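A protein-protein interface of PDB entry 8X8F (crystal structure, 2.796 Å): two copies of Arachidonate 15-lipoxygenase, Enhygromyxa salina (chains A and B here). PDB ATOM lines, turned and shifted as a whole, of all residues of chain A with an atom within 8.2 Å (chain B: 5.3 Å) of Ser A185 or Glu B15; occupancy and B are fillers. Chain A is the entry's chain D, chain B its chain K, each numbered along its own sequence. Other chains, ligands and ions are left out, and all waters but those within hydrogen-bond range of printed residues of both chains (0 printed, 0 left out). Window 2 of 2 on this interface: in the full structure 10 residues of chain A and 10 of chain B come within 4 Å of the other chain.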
ATOM      1  N   ARG A 182      23.321  -5.068   5.820  1.00  0.00           N
ATOM      2  CA  ARG A 182      23.910  -5.205   4.499  1.00  0.00           C
ATOM      3  C   ARG A 182      24.103  -3.839   3.845  1.00  0.00           C
ATOM      4  O   ARG A 182      23.420  -2.871   4.188  1.00  0.00           O
ATOM      5  CB  ARG A 182      23.029  -6.096   3.627  1.00  0.00           C
ATOM      6  CG  ARG A 182      22.940  -7.536   4.112  1.00  0.00           C
ATOM      7  CD  ARG A 182      24.320  -8.112   4.415  1.00  0.00           C
ATOM      8  NE  ARG A 182      25.223  -8.033   3.270  1.00  0.00           N
ATOM      9  CZ  ARG A 182      26.472  -8.491   3.268  1.00  0.00           C
ATOM     10  NH1 ARG A 182      26.972  -9.067   4.353  1.00  0.00           N
ATOM     11  NH2 ARG A 182      27.221  -8.374   2.183  1.00  0.00           N
ATOM     12  N   PRO A 183      25.039  -3.733   2.899  1.00  0.00           N
ATOM     13  CA  PRO A 183      25.356  -2.426   2.312  1.00  0.00           C
ATOM     14  C   PRO A 183      24.498  -2.070   1.108  1.00  0.00           C
ATOM     15  O   PRO A 183      24.144  -2.915   0.282  1.00  0.00           O
ATOM     16  CB  PRO A 183      26.823  -2.598   1.895  1.00  0.00           C
ATOM     17  CG  PRO A 183      26.913  -4.037   1.516  1.00  0.00           C
ATOM     18  CD  PRO A 183      25.971  -4.780   2.438  1.00  0.00           C
ATOM     19  N   GLN A 184      24.166  -0.779   1.013  1.00  0.00           N
ATOM     20  CA  GLN A 184      23.506  -0.266  -0.184  1.00  0.00           C
ATOM     21  C   GLN A 184      24.479  -0.207  -1.354  1.00  0.00           C
ATOM     22  O   GLN A 184      24.169  -0.672  -2.458  1.00  0.00           O
ATOM     23  CB  GLN A 184      22.914   1.118   0.090  1.00  0.00           C
ATOM     24  CG  GLN A 184      21.396   1.149   0.151  1.00  0.00           C
ATOM     25  CD  GLN A 184      20.851   0.544   1.428  1.00  0.00           C
ATOM     26  OE1 GLN A 184      21.163   1.003   2.526  1.00  0.00           O
ATOM     27  NE2 GLN A 184      20.032  -0.493   1.290  1.00  0.00           N
ATOM     28  N   SER A 185      25.662   0.367  -1.131  1.00  0.00           N
ATOM     29  CA  SER A 185      26.719   0.428  -2.131  1.00  0.00           C
ATOM     30  C   SER A 185      28.060   0.242  -1.431  1.00  0.00           C
ATOM     31  O   SER A 185      28.132   0.104  -0.206  1.00  0.00           O
ATOM     32  CB  SER A 185      26.681   1.751  -2.905  1.00  0.00           C
ATOM     33  OG  SER A 185      26.780   2.859  -2.027  1.00  0.00           O
ATOM     34  N   MET A 186      29.133   0.242  -2.219  1.00  0.00           N
ATOM     35  CA  MET A 186      30.478   0.141  -1.667  1.00  0.00           C
ATOM     36  C   MET A 186      30.978   1.457  -1.086  1.00  0.00           C
ATOM     37  O   MET A 186      32.089   1.497  -0.548  1.00  0.00           O
ATOM     38  CB  MET A 186      31.448  -0.359  -2.740  1.00  0.00           C
ATOM     39  CG  MET A 186      31.232  -1.812  -3.136  1.00  0.00           C
ATOM     40  SD  MET A 186      32.008  -2.978  -1.998  1.00  0.00           S
ATOM     41  CE  MET A 186      33.733  -2.533  -2.189  1.00  0.00           C
ATOM     42  N   ASP A 187      30.189   2.531  -1.188  1.00  0.00           N
ATOM     43  CA  ASP A 187      30.540   3.777  -0.516  1.00  0.00           C
ATOM     44  C   ASP A 187      30.365   3.662   0.990  1.00  0.00           C
ATOM     45  O   ASP A 187      31.065   4.344   1.747  1.00  0.00           O
ATOM     46  CB  ASP A 187      29.685   4.923  -1.055  1.00  0.00           C
ATOM     47  CG  ASP A 187      29.788   5.070  -2.556  1.00  0.00           C
ATOM     48  OD1 ASP A 187      29.776   4.037  -3.258  1.00  0.00           O
ATOM     49  OD2 ASP A 187      29.867   6.219  -3.035  1.00  0.00           O
ATOM     50  N   ASP A 188      29.441   2.808   1.439  1.00  0.00           N
ATOM     51  CA  ASP A 188      29.188   2.650   2.866  1.00  0.00           C
ATOM     52  C   ASP A 188      30.413   2.168   3.630  1.00  0.00           C
ATOM     53  O   ASP A 188      30.493   2.381   4.844  1.00  0.00           O
ATOM     54  CB  ASP A 188      28.035   1.671   3.091  1.00  0.00           C
ATOM     55  CG  ASP A 188      26.754   2.113   2.420  1.00  0.00           C
ATOM     56  OD1 ASP A 188      26.774   3.137   1.705  1.00  0.00           O
ATOM     57  OD2 ASP A 188      25.724   1.434   2.610  1.00  0.00           O
ATOM     58  N   TYR A 189      31.367   1.525   2.951  1.00  0.00           N
ATOM     59  CA  TYR A 189      32.537   0.992   3.641  1.00  0.00           C
ATOM     60  C   TYR A 189      33.615   2.054   3.829  1.00  0.00           C
ATOM     61  O   TYR A 189      34.239   2.123   4.894  1.00  0.00           O
ATOM     62  CB  TYR A 189      33.085  -0.218   2.883  1.00  0.00           C
ATOM     63  CG  TYR A 189      32.179  -1.418   2.995  1.00  0.00           C
ATOM     64  CD1 TYR A 189      32.062  -2.108   4.194  1.00  0.00           C
ATOM     65  CD2 TYR A 189      31.422  -1.851   1.913  1.00  0.00           C
ATOM     66  CE1 TYR A 189      31.226  -3.199   4.316  1.00  0.00           C
ATOM     67  CE2 TYR A 189      30.580  -2.946   2.024  1.00  0.00           C
ATOM     68  CZ  TYR A 189      30.487  -3.613   3.230  1.00  0.00           C
ATOM     69  OH  TYR A 189      29.654  -4.704   3.352  1.00  0.00           O
ATOM     70  N   ALA A 190      33.849   2.889   2.814  1.00  0.00           N
ATOM     71  CA  ALA A 190      34.782   3.998   2.986  1.00  0.00           C
ATOM     72  C   ALA A 190      34.194   5.075   3.887  1.00  0.00           C
ATOM     73  O   ALA A 190      34.912   5.678   4.693  1.00  0.00           O
ATOM     74  CB  ALA A 190      35.162   4.582   1.626  1.00  0.00           C
ATOM     75  N   ASN A 191      32.883   5.317   3.780  1.00  0.00           N
ATOM     76  CA  ASN A 191      32.228   6.374   4.545  1.00  0.00           C
ATOM     77  C   ASN A 191      32.292   6.159   6.051  1.00  0.00           C
ATOM     78  O   ASN A 191      31.941   7.076   6.800  1.00  0.00           O
ATOM     79  CB  ASN A 191      30.762   6.505   4.125  1.00  0.00           C
ATOM     80  CG  ASN A 191      30.583   7.358   2.886  1.00  0.00           C
ATOM     81  OD1 ASN A 191      30.774   8.574   2.926  1.00  0.00           O
ATOM     82  ND2 ASN A 191      30.201   6.729   1.782  1.00  0.00           N
ATOM     83  N   LEU A 559      30.276  -7.218  -5.600  1.00  0.00           N
ATOM     84  CA  LEU A 559      31.392  -7.359  -4.669  1.00  0.00           C
ATOM     85  C   LEU A 559      30.982  -7.063  -3.232  1.00  0.00           C
ATOM     86  O   LEU A 559      31.586  -7.600  -2.296  1.00  0.00           O
ATOM     87  CB  LEU A 559      32.543  -6.440  -5.090  1.00  0.00           C
ATOM     88  CG  LEU A 559      33.808  -6.452  -4.228  1.00  0.00           C
ATOM     89  CD1 LEU A 559      34.557  -7.774  -4.357  1.00  0.00           C
ATOM     90  CD2 LEU A 559      34.708  -5.277  -4.581  1.00  0.00           C
ATOM     91  N   LYS A 560      29.968  -6.219  -3.034  1.00  0.00           N
ATOM     92  CA  LYS A 560      29.562  -5.849  -1.683  1.00  0.00           C
ATOM     93  C   LYS A 560      28.992  -7.026  -0.901  1.00  0.00           C
ATOM     94  O   LYS A 560      29.018  -7.001   0.334  1.00  0.00           O
ATOM     95  CB  LYS A 560      28.539  -4.711  -1.726  1.00  0.00           C
ATOM     96  CG  LYS A 560      27.327  -4.984  -2.601  1.00  0.00           C
ATOM     97  CD  LYS A 560      26.185  -4.027  -2.291  1.00  0.00           C
ATOM     98  CE  LYS A 560      25.084  -4.125  -3.336  1.00  0.00           C
ATOM     99  NZ  LYS A 560      24.649  -5.533  -3.551  1.00  0.00           N
ATOM    100  N   GLN A 563      31.628  -8.573   1.273  1.00  0.00           N
ATOM    101  CA  GLN A 563      32.125  -7.751   2.362  1.00  0.00           C
ATOM    102  C   GLN A 563      31.306  -7.972   3.632  1.00  0.00           C
ATOM    103  O   GLN A 563      30.156  -8.415   3.573  1.00  0.00           O
ATOM    104  CB  GLN A 563      32.096  -6.281   1.953  1.00  0.00           C
ATOM    105  CG  GLN A 563      32.646  -6.012   0.559  1.00  0.00           C
ATOM    106  CD  GLN A 563      34.040  -6.577   0.355  1.00  0.00           C
ATOM    107  OE1 GLN A 563      34.851  -6.618   1.279  1.00  0.00           O
ATOM    108  NE2 GLN A 563      34.324  -7.021  -0.866  1.00  0.00           N
ATOM    109  N   LEU A 566      27.848  -3.966   8.068  1.00  0.00           N
ATOM    110  CA  LEU A 566      28.368  -2.651   8.427  1.00  0.00           C
ATOM    111  C   LEU A 566      28.746  -2.577   9.901  1.00  0.00           C
ATOM    112  O   LEU A 566      29.783  -2.000  10.248  1.00  0.00           O
ATOM    113  CB  LEU A 566      27.351  -1.566   8.076  1.00  0.00           C
ATOM    114  CG  LEU A 566      27.124  -1.352   6.577  1.00  0.00           C
ATOM    115  CD1 LEU A 566      26.264  -0.124   6.329  1.00  0.00           C
ATOM    116  CD2 LEU A 566      28.452  -1.246   5.834  1.00  0.00           C
ATOM    117  N   ARG B  13      34.544   4.995  -3.435  1.00  0.00           N
ATOM    118  CA  ARG B  13      33.135   5.388  -3.363  1.00  0.00           C
ATOM    119  C   ARG B  13      32.566   5.456  -4.774  1.00  0.00           C
ATOM    120  O   ARG B  13      32.308   6.540  -5.309  1.00  0.00           O
ATOM    121  CB  ARG B  13      32.982   6.725  -2.634  1.00  0.00           C
ATOM    122  CG  ARG B  13      33.467   6.716  -1.193  1.00  0.00           C
ATOM    123  CD  ARG B  13      34.460   7.840  -0.944  1.00  0.00           C
ATOM    124  NE  ARG B  13      34.874   7.907   0.455  1.00  0.00           N
ATOM    125  CZ  ARG B  13      34.253   8.631   1.378  1.00  0.00           C
ATOM    126  NH1 ARG B  13      33.187   9.351   1.053  1.00  0.00           N
ATOM    127  NH2 ARG B  13      34.697   8.635   2.628  1.00  0.00           N
ATOM    128  N   PRO B  14      32.348   4.300  -5.411  1.00  0.00           N
ATOM    129  CA  PRO B  14      31.933   4.326  -6.826  1.00  0.00           C
ATOM    130  C   PRO B  14      30.546   4.900  -7.056  1.00  0.00           C
ATOM    131  O   PRO B  14      30.353   5.640  -8.028  1.00  0.00           O
ATOM    132  CB  PRO B  14      32.009   2.846  -7.238  1.00  0.00           C
ATOM    133  CG  PRO B  14      32.906   2.204  -6.229  1.00  0.00           C
ATOM    134  CD  PRO B  14      32.637   2.932  -4.948  1.00  0.00           C
ATOM    135  N   GLU B  15      29.572   4.580  -6.198  1.00  0.00           N
ATOM    136  CA  GLU B  15      28.200   5.021  -6.441  1.00  0.00           C
ATOM    137  C   GLU B  15      28.092   6.541  -6.470  1.00  0.00           C
ATOM    138  O   GLU B  15      27.323   7.100  -7.261  1.00  0.00           O
ATOM    139  CB  GLU B  15      27.264   4.440  -5.378  1.00  0.00           C
ATOM    140  CG  GLU B  15      25.786   4.548  -5.727  1.00  0.00           C
ATOM    141  CD  GLU B  15      25.273   3.334  -6.478  1.00  0.00           C
ATOM    142  OE1 GLU B  15      25.130   2.265  -5.847  1.00  0.00           O
ATOM    143  OE2 GLU B  15      25.025   3.446  -7.697  1.00  0.00           O
ATOM    144  N   GLN B  16      28.852   7.227  -5.612  1.00  0.00           N
ATOM    145  CA  GLN B  16      28.850   8.686  -5.622  1.00  0.00           C
ATOM    146  C   GLN B  16      29.484   9.228  -6.896  1.00  0.00           C
ATOM    147  O   GLN B  16      29.031  10.241  -7.442  1.00  0.00           O
ATOM    148  CB  GLN B  16      29.589   9.213  -4.393  1.00  0.00           C
ATOM    149  CG  GLN B  16      29.595  10.726  -4.258  1.00  0.00           C
ATOM    150  CD  GLN B  16      30.804  11.223  -3.494  1.00  0.00           C
ATOM    151  OE1 GLN B  16      31.942  10.933  -3.861  1.00  0.00           O
ATOM    152  NE2 GLN B  16      30.564  11.963  -2.417  1.00  0.00           N
ATOM    153  N   ARG B  17      30.542   8.571  -7.372  1.00  0.00           N
ATOM    154  CA  ARG B  17      31.178   8.974  -8.622  1.00  0.00           C
ATOM    155  C   ARG B  17      30.206   8.863  -9.791  1.00  0.00           C
ATOM    156  O   ARG B  17      30.179   9.733 -10.671  1.00  0.00           O
ATOM    157  CB  ARG B  17      32.417   8.110  -8.859  1.00  0.00           C
ATOM    158  CG  ARG B  17      33.191   8.389 -10.135  1.00  0.00           C
ATOM    159  CD  ARG B  17      34.077   7.203 -10.475  1.00  0.00           C
ATOM    160  NE  ARG B  17      35.203   7.558 -11.333  1.00  0.00           N
ATOM    161  CZ  ARG B  17      36.403   7.910 -10.880  1.00  0.00           C
ATOM    162  NH1 ARG B  17      36.633   7.961  -9.575  1.00  0.00           N
ATOM    163  NH2 ARG B  17      37.375   8.211 -11.728  1.00  0.00           N
ATOM    164  N   ALA B  18      29.393   7.803  -9.813  1.00  0.00           N
ATOM    165  CA  ALA B  18      28.432   7.633 -10.897  1.00  0.00           C
ATOM    166  C   ALA B  18      27.317   8.667 -10.830  1.00  0.00           C
ATOM    167  O   ALA B  18      26.769   9.053 -11.869  1.00  0.00           O
ATOM    168  CB  ALA B  18      27.843   6.224 -10.868  1.00  0.00           C
ATOM    169  N   GLN B  19      26.960   9.119  -9.626  1.00  0.00           N
ATOM    170  CA  GLN B  19      25.908  10.122  -9.503  1.00  0.00           C
ATOM    171  C   GLN B  19      26.382  11.488  -9.976  1.00  0.00           C
ATOM    172  O   GLN B  19      25.582  12.276 -10.492  1.00  0.00           O
ATOM    173  CB  GLN B  19      25.412  10.196  -8.059  1.00  0.00           C
ATOM    174  CG  GLN B  19      24.691   8.942  -7.590  1.00  0.00           C
ATOM    175  CD  GLN B  19      24.117   9.084  -6.194  1.00  0.00           C
ATOM    176  OE1 GLN B  19      24.157  10.162  -5.600  1.00  0.00           O
ATOM    177  NE2 GLN B  19      23.579   7.992  -5.660  1.00  0.00           N
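Hydrophobic or aromatic side chains of chain B that line the printed part of chain A: Pro B14.
Among the printed residues, 7 pairs touch across the chains.
Among the printed residues, no Asp or Glu carboxylate lies within 4 Å of a Lys or Arg side-chain nitrogen of the other chain.
No position is printed for both chains.
Of the 7 pairs that touch across the chains among the printed residues, none has its exchanged pair printed and touching as well.
Ser A185 touches just one residue of chain B: Glu B15.
Glu B15 touches just these residues of chain A: Ser A185 and Asp A187.
Of the printed residues of chain B, Asp A187 touches Arg B13, Pro B14, Glu B15 and Gln B16.
Of the printed residues of chain A, Arg B13 touches Asp A187, Ala A190 and Asn A191.
Of the printed residues of chain A, Gln B16 touches Asp A187.
Of the printed residues of chain B, Ala A190 touches Arg B13 (3.5 Å).
Gln A563 touches none of the printed residues of chain B.
Gln B19 touches none of the printed residues of chain A.
The nearest printed residue of chain B that does not touch Ser A185 is Gln B16 (6.0 Å).
The nearest residue of chain A that does not touch Glu B15 is Gln A184 (4.6 Å).
The side-chain hydroxyl (OG) of Ser A185 is in hydrogen-bond range of the side-chain carboxylate (OD1) of Asp A187, 3.4 Å away.
O of Asp A187 lies within hydrogen-bond range of ND2 of Asn A191.
Among the printed residues, pairs that only touch across the chains: Ser A185 with Glu B15 (3.4 Å) and Ala A190 with Arg B13 (3.5 Å).
The backbone NH of Glu B15 is in hydrogen-bond range of the side-chain carboxylate of Asp A187, 3.0 Å away.
N of Gln B16 sits at hydrogen-bond distance from OD2 of Asp A187, at 2.9 Å.
The side-chain amide oxygen of Asn A191 is in hydrogen-bond range of the guanidinium group of Arg B13.
The side-chain carboxylate (OD2) of Asp A187 sits close to the backbone carbonyl oxygen (O) of Arg B13 (3.4 Å).
The side-chain carboxylate of Asp A187 sits close to the backbone nitrogen of Pro B14 (3.4 Å).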
